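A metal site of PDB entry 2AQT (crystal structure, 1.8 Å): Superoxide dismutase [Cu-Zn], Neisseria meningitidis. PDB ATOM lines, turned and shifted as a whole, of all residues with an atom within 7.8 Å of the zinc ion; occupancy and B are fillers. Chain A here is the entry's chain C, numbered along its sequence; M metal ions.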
ATOM      1  N   PHE A  56     -23.624   5.816 -23.982  1.00  0.00           N
ATOM      2  CA  PHE A  56     -24.100   6.701 -22.921  1.00  0.00           C
ATOM      3  C   PHE A  56     -24.667   7.985 -23.564  1.00  0.00           C
ATOM      4  O   PHE A  56     -23.912   8.792 -24.090  1.00  0.00           O
ATOM      5  CB  PHE A  56     -22.885   6.998 -22.044  1.00  0.00           C
ATOM      6  CG  PHE A  56     -23.194   7.642 -20.723  1.00  0.00           C
ATOM      7  CD1 PHE A  56     -24.274   7.215 -19.958  1.00  0.00           C
ATOM      8  CD2 PHE A  56     -22.338   8.603 -20.200  1.00  0.00           C
ATOM      9  CE1 PHE A  56     -24.481   7.728 -18.680  1.00  0.00           C
ATOM     10  CE2 PHE A  56     -22.532   9.125 -18.937  1.00  0.00           C
ATOM     11  CZ  PHE A  56     -23.604   8.690 -18.163  1.00  0.00           C
ATOM     12  N   HIS A  57     -25.995   8.153 -23.531  1.00  0.00           N
ATOM     13  CA  HIS A  57     -26.608   9.336 -24.143  1.00  0.00           C
ATOM     14  C   HIS A  57     -27.757   9.939 -23.352  1.00  0.00           C
ATOM     15  O   HIS A  57     -28.368   9.289 -22.502  1.00  0.00           O
ATOM     16  CB  HIS A  57     -27.171   9.009 -25.536  1.00  0.00           C
ATOM     17  CG  HIS A  57     -26.442   7.917 -26.258  1.00  0.00           C
ATOM     18  ND1 HIS A  57     -27.007   6.682 -26.487  1.00  0.00           N
ATOM     19  CD2 HIS A  57     -25.205   7.887 -26.817  1.00  0.00           C
ATOM     20  CE1 HIS A  57     -26.145   5.930 -27.150  1.00  0.00           C
ATOM     21  NE2 HIS A  57     -25.047   6.635 -27.367  1.00  0.00           N
ATOM     22  N   ILE A  58     -28.040  11.197 -23.637  1.00  0.00           N
ATOM     23  CA  ILE A  58     -29.183  11.859 -23.023  1.00  0.00           C
ATOM     24  C   ILE A  58     -30.297  11.657 -24.049  1.00  0.00           C
ATOM     25  O   ILE A  58     -30.108  11.957 -25.230  1.00  0.00           O
ATOM     26  CB  ILE A  58     -28.953  13.379 -22.840  1.00  0.00           C
ATOM     27  CG1 ILE A  58     -27.763  13.631 -21.913  1.00  0.00           C
ATOM     28  CG2 ILE A  58     -30.214  14.030 -22.280  1.00  0.00           C
ATOM     29  CD1 ILE A  58     -27.923  13.012 -20.543  1.00  0.00           C
ATOM     30  N   HIS A  59     -31.435  11.133 -23.608  1.00  0.00           N
ATOM     31  CA  HIS A  59     -32.559  10.922 -24.510  1.00  0.00           C
ATOM     32  C   HIS A  59     -33.612  12.003 -24.334  1.00  0.00           C
ATOM     33  O   HIS A  59     -33.713  12.640 -23.274  1.00  0.00           O
ATOM     34  CB  HIS A  59     -33.139   9.510 -24.312  1.00  0.00           C
ATOM     35  CG  HIS A  59     -32.329   8.439 -24.963  1.00  0.00           C
ATOM     36  ND1 HIS A  59     -32.847   7.568 -25.895  1.00  0.00           N
ATOM     37  CD2 HIS A  59     -31.017   8.122 -24.854  1.00  0.00           C
ATOM     38  CE1 HIS A  59     -31.894   6.765 -26.336  1.00  0.00           C
ATOM     39  NE2 HIS A  59     -30.773   7.085 -25.726  1.00  0.00           N
ATOM     40  N   GLY A  81     -35.903   9.052 -28.669  1.00  0.00           N
ATOM     41  CA  GLY A  81     -34.574   8.958 -29.241  1.00  0.00           C
ATOM     42  C   GLY A  81     -33.520   9.821 -28.582  1.00  0.00           C
ATOM     43  O   GLY A  81     -33.759  10.423 -27.523  1.00  0.00           O
ATOM     44  N   HIS A  82     -32.355   9.886 -29.198  1.00  0.00           N
ATOM     45  CA  HIS A  82     -31.271  10.706 -28.681  1.00  0.00           C
ATOM     46  C   HIS A  82     -31.718  12.155 -28.670  1.00  0.00           C
ATOM     47  O   HIS A  82     -32.275  12.650 -29.658  1.00  0.00           O
ATOM     48  CB  HIS A  82     -30.020  10.560 -29.542  1.00  0.00           C
ATOM     49  CG  HIS A  82     -29.372   9.210 -29.459  1.00  0.00           C
ATOM     50  ND1 HIS A  82     -28.064   8.990 -29.822  1.00  0.00           N
ATOM     51  CD2 HIS A  82     -29.861   8.011 -29.043  1.00  0.00           C
ATOM     52  CE1 HIS A  82     -27.770   7.717 -29.627  1.00  0.00           C
ATOM     53  NE2 HIS A  82     -28.835   7.103 -29.158  1.00  0.00           N
ATOM     54  N   TRP A  83     -31.498  12.837 -27.545  1.00  0.00           N
ATOM     55  CA  TRP A  83     -31.874  14.245 -27.409  1.00  0.00           C
ATOM     56  C   TRP A  83     -31.207  15.036 -28.519  1.00  0.00           C
ATOM     57  O   TRP A  83     -29.980  15.103 -28.607  1.00  0.00           O
ATOM     58  CB  TRP A  83     -31.443  14.741 -26.024  1.00  0.00           C
ATOM     59  CG  TRP A  83     -31.886  16.134 -25.709  1.00  0.00           C
ATOM     60  CD1 TRP A  83     -33.112  16.688 -25.964  1.00  0.00           C
ATOM     61  CD2 TRP A  83     -31.131  17.117 -25.015  1.00  0.00           C
ATOM     62  NE1 TRP A  83     -33.158  17.971 -25.472  1.00  0.00           N
ATOM     63  CE2 TRP A  83     -31.948  18.265 -24.882  1.00  0.00           C
ATOM     64  CE3 TRP A  83     -29.827  17.152 -24.496  1.00  0.00           C
ATOM     65  CZ2 TRP A  83     -31.523  19.430 -24.237  1.00  0.00           C
ATOM     66  CZ3 TRP A  83     -29.402  18.317 -23.851  1.00  0.00           C
ATOM     67  CH2 TRP A  83     -30.245  19.440 -23.729  1.00  0.00           C
ATOM     68  N   ASP A  84     -32.011  15.677 -29.359  1.00  0.00           N
ATOM     69  CA  ASP A  84     -31.492  16.405 -30.508  1.00  0.00           C
ATOM     70  C   ASP A  84     -32.251  17.713 -30.754  1.00  0.00           C
ATOM     71  O   ASP A  84     -32.871  17.885 -31.802  1.00  0.00           O
ATOM     72  CB  ASP A  84     -31.575  15.456 -31.715  1.00  0.00           C
ATOM     73  CG  ASP A  84     -30.965  16.032 -32.962  1.00  0.00           C
ATOM     74  OD1 ASP A  84     -29.982  16.792 -32.878  1.00  0.00           O
ATOM     75  OD2 ASP A  84     -31.464  15.685 -34.060  1.00  0.00           O
ATOM     76  N   LYS A  89     -29.828  15.413 -36.361  1.00  0.00           N
ATOM     77  CA  LYS A  89     -30.355  14.201 -36.981  1.00  0.00           C
ATOM     78  C   LYS A  89     -29.326  13.126 -37.332  1.00  0.00           C
ATOM     79  O   LYS A  89     -29.558  12.295 -38.208  1.00  0.00           O
ATOM     80  CB  LYS A  89     -31.176  14.572 -38.219  1.00  0.00           C
ATOM     81  CG  LYS A  89     -32.477  15.264 -37.855  1.00  0.00           C
ATOM     82  CD  LYS A  89     -33.289  15.681 -39.072  1.00  0.00           C
ATOM     83  CE  LYS A  89     -34.674  16.138 -38.662  1.00  0.00           C
ATOM     84  NZ  LYS A  89     -34.622  17.134 -37.567  1.00  0.00           N
ATOM     85  N   GLN A  90     -28.189  13.146 -36.639  1.00  0.00           N
ATOM     86  CA  GLN A  90     -27.171  12.137 -36.844  1.00  0.00           C
ATOM     87  C   GLN A  90     -26.391  11.935 -35.560  1.00  0.00           C
ATOM     88  O   GLN A  90     -26.237  12.855 -34.762  1.00  0.00           O
ATOM     89  CB  GLN A  90     -26.223  12.512 -37.987  1.00  0.00           C
ATOM     90  CG  GLN A  90     -25.348  13.714 -37.773  1.00  0.00           C
ATOM     91  CD  GLN A  90     -24.299  13.863 -38.863  1.00  0.00           C
ATOM     92  OE1 GLN A  90     -24.626  13.864 -40.052  1.00  0.00           O
ATOM     93  NE2 GLN A  90     -23.045  13.993 -38.464  1.00  0.00           N
ATOM     94  N   HIS A  91     -25.911  10.713 -35.358  1.00  0.00           N
ATOM     95  CA  HIS A  91     -25.157  10.377 -34.166  1.00  0.00           C
ATOM     96  C   HIS A  91     -23.680  10.671 -34.383  1.00  0.00           C
ATOM     97  O   HIS A  91     -23.152  10.438 -35.480  1.00  0.00           O
ATOM     98  CB  HIS A  91     -25.357   8.899 -33.815  1.00  0.00           C
ATOM     99  CG  HIS A  91     -24.713   8.499 -32.530  1.00  0.00           C
ATOM    100  ND1 HIS A  91     -25.160   8.938 -31.301  1.00  0.00           N
ATOM    101  CD2 HIS A  91     -23.640   7.714 -32.277  1.00  0.00           C
ATOM    102  CE1 HIS A  91     -24.395   8.436 -30.352  1.00  0.00           C
ATOM    103  NE2 HIS A  91     -23.466   7.690 -30.911  1.00  0.00           N
ATOM    104  N   GLY A  92     -23.012  11.184 -33.364  1.00  0.00           N
ATOM    105  CA  GLY A  92     -21.603  11.485 -33.506  1.00  0.00           C
ATOM    106  C   GLY A  92     -20.868  11.620 -32.192  1.00  0.00           C
ATOM    107  O   GLY A  92     -21.260  11.020 -31.196  1.00  0.00           O
ATOM    108  N   TYR A  93     -19.806  12.409 -32.217  1.00  0.00           N
ATOM    109  CA  TYR A  93     -18.949  12.643 -31.044  1.00  0.00           C
ATOM    110  C   TYR A  93     -19.489  13.702 -30.112  1.00  0.00           C
ATOM    111  O   TYR A  93     -20.253  14.577 -30.539  1.00  0.00           O
ATOM    112  CB  TYR A  93     -17.555  13.045 -31.508  1.00  0.00           C
ATOM    113  CG  TYR A  93     -16.810  11.951 -32.244  1.00  0.00           C
ATOM    114  CD1 TYR A  93     -16.194  10.917 -31.551  1.00  0.00           C
ATOM    115  CD2 TYR A  93     -16.740  11.955 -33.637  1.00  0.00           C
ATOM    116  CE1 TYR A  93     -15.523   9.898 -32.225  1.00  0.00           C
ATOM    117  CE2 TYR A  93     -16.076  10.934 -34.319  1.00  0.00           C
ATOM    118  CZ  TYR A  93     -15.470   9.922 -33.609  1.00  0.00           C
ATOM    119  OH  TYR A  93     -14.808   8.914 -34.278  1.00  0.00           O
ATOM    120  N   ALA A  99     -23.808  16.744 -34.310  1.00  0.00           N
ATOM    121  CA  ALA A  99     -24.197  15.446 -33.763  1.00  0.00           C
ATOM    122  C   ALA A  99     -25.284  15.733 -32.732  1.00  0.00           C
ATOM    123  O   ALA A  99     -25.441  16.879 -32.308  1.00  0.00           O
ATOM    124  CB  ALA A  99     -22.992  14.771 -33.106  1.00  0.00           C
ATOM    125  N   HIS A 100     -26.039  14.704 -32.353  1.00  0.00           N
ATOM    126  CA  HIS A 100     -27.096  14.857 -31.340  1.00  0.00           C
ATOM    127  C   HIS A 100     -26.482  15.554 -30.126  1.00  0.00           C
ATOM    128  O   HIS A 100     -25.402  15.176 -29.673  1.00  0.00           O
ATOM    129  CB  HIS A 100     -27.603  13.489 -30.887  1.00  0.00           C
ATOM    130  CG  HIS A 100     -28.185  12.654 -31.981  1.00  0.00           C
ATOM    131  ND1 HIS A 100     -27.980  11.298 -32.070  1.00  0.00           N
ATOM    132  CD2 HIS A 100     -29.020  12.971 -33.008  1.00  0.00           C
ATOM    133  CE1 HIS A 100     -28.658  10.805 -33.087  1.00  0.00           C
ATOM    134  NE2 HIS A 100     -29.302  11.806 -33.674  1.00  0.00           N
ATOM    135  N   LEU A 101     -27.161  16.558 -29.579  1.00  0.00           N
ATOM    136  CA  LEU A 101     -26.624  17.251 -28.405  1.00  0.00           C
ATOM    137  C   LEU A 101     -26.519  16.275 -27.223  1.00  0.00           C
ATOM    138  O   LEU A 101     -25.746  16.497 -26.289  1.00  0.00           O
ATOM    139  CB  LEU A 101     -27.530  18.427 -28.015  1.00  0.00           C
ATOM    140  CG  LEU A 101     -27.000  19.348 -26.926  1.00  0.00           C
ATOM    141  CD1 LEU A 101     -25.728  20.024 -27.395  1.00  0.00           C
ATOM    142  CD2 LEU A 101     -28.061  20.387 -26.591  1.00  0.00           C
ATOM    143  N   GLY A 102     -27.299  15.203 -27.283  1.00  0.00           N
ATOM    144  CA  GLY A 102     -27.298  14.227 -26.214  1.00  0.00           C
ATOM    145  C   GLY A 102     -26.189  13.187 -26.258  1.00  0.00           C
ATOM    146  O   GLY A 102     -26.116  12.324 -25.386  1.00  0.00           O
ATOM    147  N   ASP A 103     -25.332  13.246 -27.284  1.00  0.00           N
ATOM    148  CA  ASP A 103     -24.242  12.272 -27.399  1.00  0.00           C
ATOM    149  C   ASP A 103     -23.118  12.530 -26.411  1.00  0.00           C
ATOM    150  O   ASP A 103     -22.314  13.439 -26.579  1.00  0.00           O
ATOM    151  CB  ASP A 103     -23.693  12.269 -28.817  1.00  0.00           C
ATOM    152  CG  ASP A 103     -24.738  11.812 -29.822  1.00  0.00           C
ATOM    153  OD1 ASP A 103     -25.714  11.170 -29.387  1.00  0.00           O
ATOM    154  OD2 ASP A 103     -24.561  12.095 -31.030  1.00  0.00           O
ATOM    155  N   LEU A 104     -23.045  11.687 -25.377  1.00  0.00           N
ATOM    156  CA  LEU A 104     -22.023  11.810 -24.341  1.00  0.00           C
ATOM    157  C   LEU A 104     -20.866  10.849 -24.591  1.00  0.00           C
ATOM    158  O   LEU A 104     -20.970   9.927 -25.422  1.00  0.00           O
ATOM    159  CB  LEU A 104     -22.641  11.481 -22.974  1.00  0.00           C
ATOM    160  CG  LEU A 104     -23.918  12.181 -22.524  1.00  0.00           C
ATOM    161  CD1 LEU A 104     -24.322  11.648 -21.159  1.00  0.00           C
ATOM    162  CD2 LEU A 104     -23.704  13.686 -22.462  1.00  0.00           C
ATOM    163  N   ARG A 123     -20.460  20.375 -24.980  1.00  0.00           N
ATOM    164  CA  ARG A 123     -21.534  21.142 -25.604  1.00  0.00           C
ATOM    165  C   ARG A 123     -22.699  21.462 -24.677  1.00  0.00           C
ATOM    166  O   ARG A 123     -23.633  22.183 -25.070  1.00  0.00           O
ATOM    167  CB  ARG A 123     -22.044  20.408 -26.849  1.00  0.00           C
ATOM    168  CG  ARG A 123     -21.052  20.376 -28.003  1.00  0.00           C
ATOM    169  CD  ARG A 123     -21.687  19.760 -29.261  1.00  0.00           C
ATOM    170  NE  ARG A 123     -21.833  18.304 -29.149  1.00  0.00           N
ATOM    171  CZ  ARG A 123     -22.839  17.613 -29.678  1.00  0.00           C
ATOM    172  NH1 ARG A 123     -23.802  18.228 -30.348  1.00  0.00           N
ATOM    173  NH2 ARG A 123     -22.878  16.284 -29.547  1.00  0.00           N
ATOM    174  N   ASP A 142     -20.187   2.492 -28.224  1.00  0.00           N
ATOM    175  CA  ASP A 142     -20.506   3.697 -28.990  1.00  0.00           C
ATOM    176  C   ASP A 142     -19.291   4.140 -29.801  1.00  0.00           C
ATOM    177  O   ASP A 142     -18.302   4.643 -29.232  1.00  0.00           O
ATOM    178  CB  ASP A 142     -20.933   4.822 -28.042  1.00  0.00           C
ATOM    179  CG  ASP A 142     -21.591   5.988 -28.776  1.00  0.00           C
ATOM    180  OD1 ASP A 142     -21.481   6.045 -30.011  1.00  0.00           O
ATOM    181  OD2 ASP A 142     -22.221   6.836 -28.105  1.00  0.00           O
ATOM    182  N   HIS A 144     -19.507   6.430 -31.932  1.00  0.00           N
ATOM    183  CA  HIS A 144     -19.878   7.805 -32.308  1.00  0.00           C
ATOM    184  C   HIS A 144     -20.125   8.004 -33.795  1.00  0.00           C
ATOM    185  O   HIS A 144     -19.656   8.972 -34.393  1.00  0.00           O
ATOM    186  CB  HIS A 144     -18.787   8.772 -31.824  1.00  0.00           C
ATOM    187  CG  HIS A 144     -18.603   8.760 -30.345  1.00  0.00           C
ATOM    188  ND1 HIS A 144     -19.591   9.160 -29.467  1.00  0.00           N
ATOM    189  CD2 HIS A 144     -17.554   8.377 -29.569  1.00  0.00           C
ATOM    190  CE1 HIS A 144     -19.173   9.025 -28.227  1.00  0.00           C
ATOM    191  NE2 HIS A 144     -17.933   8.552 -28.259  1.00  0.00           N
ATOM    192  N   SER A 145     -20.877   7.084 -34.371  1.00  0.00           N
ATOM    193  CA  SER A 145     -21.190   7.156 -35.788  1.00  0.00           C
ATOM    194  C   SER A 145     -22.414   6.305 -36.069  1.00  0.00           C
ATOM    195  O   SER A 145     -22.773   5.449 -35.255  1.00  0.00           O
ATOM    196  CB  SER A 145     -20.014   6.648 -36.630  1.00  0.00           C
ATOM    197  OG  SER A 145     -20.351   6.593 -38.004  1.00  0.00           O
ATOM    198  N   ASP A 146     -23.061   6.560 -37.198  1.00  0.00           N
ATOM    199  CA  ASP A 146     -24.224   5.768 -37.580  1.00  0.00           C
ATOM    200  C   ASP A 146     -23.756   4.653 -38.498  1.00  0.00           C
ATOM    201  O   ASP A 146     -24.556   3.899 -39.035  1.00  0.00           O
ATOM    202  CB  ASP A 146     -25.263   6.626 -38.276  1.00  0.00           C
ATOM    203  CG  ASP A 146     -26.007   7.526 -37.318  1.00  0.00           C
ATOM    204  OD1 ASP A 146     -26.655   7.001 -36.385  1.00  0.00           O
ATOM    205  OD2 ASP A 146     -25.936   8.761 -37.481  1.00  0.00           O
ATOM    206  N   LEU A 151     -26.820   4.733 -34.421  1.00  0.00           N
ATOM    207  CA  LEU A 151     -26.648   5.275 -33.086  1.00  0.00           C
ATOM    208  C   LEU A 151     -25.410   4.787 -32.317  1.00  0.00           C
ATOM    209  O   LEU A 151     -25.450   4.621 -31.102  1.00  0.00           O
ATOM    210  CB  LEU A 151     -27.916   4.989 -32.284  1.00  0.00           C
ATOM    211  CG  LEU A 151     -29.184   5.473 -32.996  1.00  0.00           C
ATOM    212  CD1 LEU A 151     -30.419   4.973 -32.262  1.00  0.00           C
ATOM    213  CD2 LEU A 151     -29.181   6.992 -33.077  1.00  0.00           C
ATOM    214  N   GLY A 152     -24.318   4.568 -33.050  1.00  0.00           N
ATOM    215  CA  GLY A 152     -23.074   4.135 -32.428  1.00  0.00           C
ATOM    216  C   GLY A 152     -22.969   2.664 -32.098  1.00  0.00           C
ATOM    217  O   GLY A 152     -21.931   2.206 -31.611  1.00  0.00           O
HETATM  218 ZN    ZN M   1     -26.775  10.236 -30.746  1.00  0.00          ZN
HETATM  219 CU    CU M   2     -28.926   6.197 -26.013  1.00  0.00          CU
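The zinc ion is bound by the side-chain carboxylate (OD1) of Asp 103 (2.0 Å), a ring nitrogen (ND1) of His 82 (2.0 Å), a ring nitrogen (ND1) of His 100 (2.1 Å) and a ring nitrogen (ND1) of His 91 (2.1 Å).
The zinc ion has four donor atoms within binding distance.
Of the 26 residues printed, 4 come within 4 Å of the zinc ion.
OD2 of Asp 103 lies within hydrogen-bond range of N of Gly 92.
A ring nitrogen (NE2) of His 82 lies close to a ring nitrogen (ND1) of His 57.
N of His 100 lies within hydrogen-bond range of O of Gln 90, at 3.0 Å.
The backbone carbonyl oxygen of His 100 lies within hydrogen-bond range of the guanidinium group of Arg 123, at 2.8 Å.
A ring nitrogen (NE2) of His 91 sits at hydrogen-bond distance from the side-chain carboxylate (OD1) of Asp 142 (2.7 Å).
OD2 of Asp 146 sits at hydrogen-bond distance from N of His 91.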
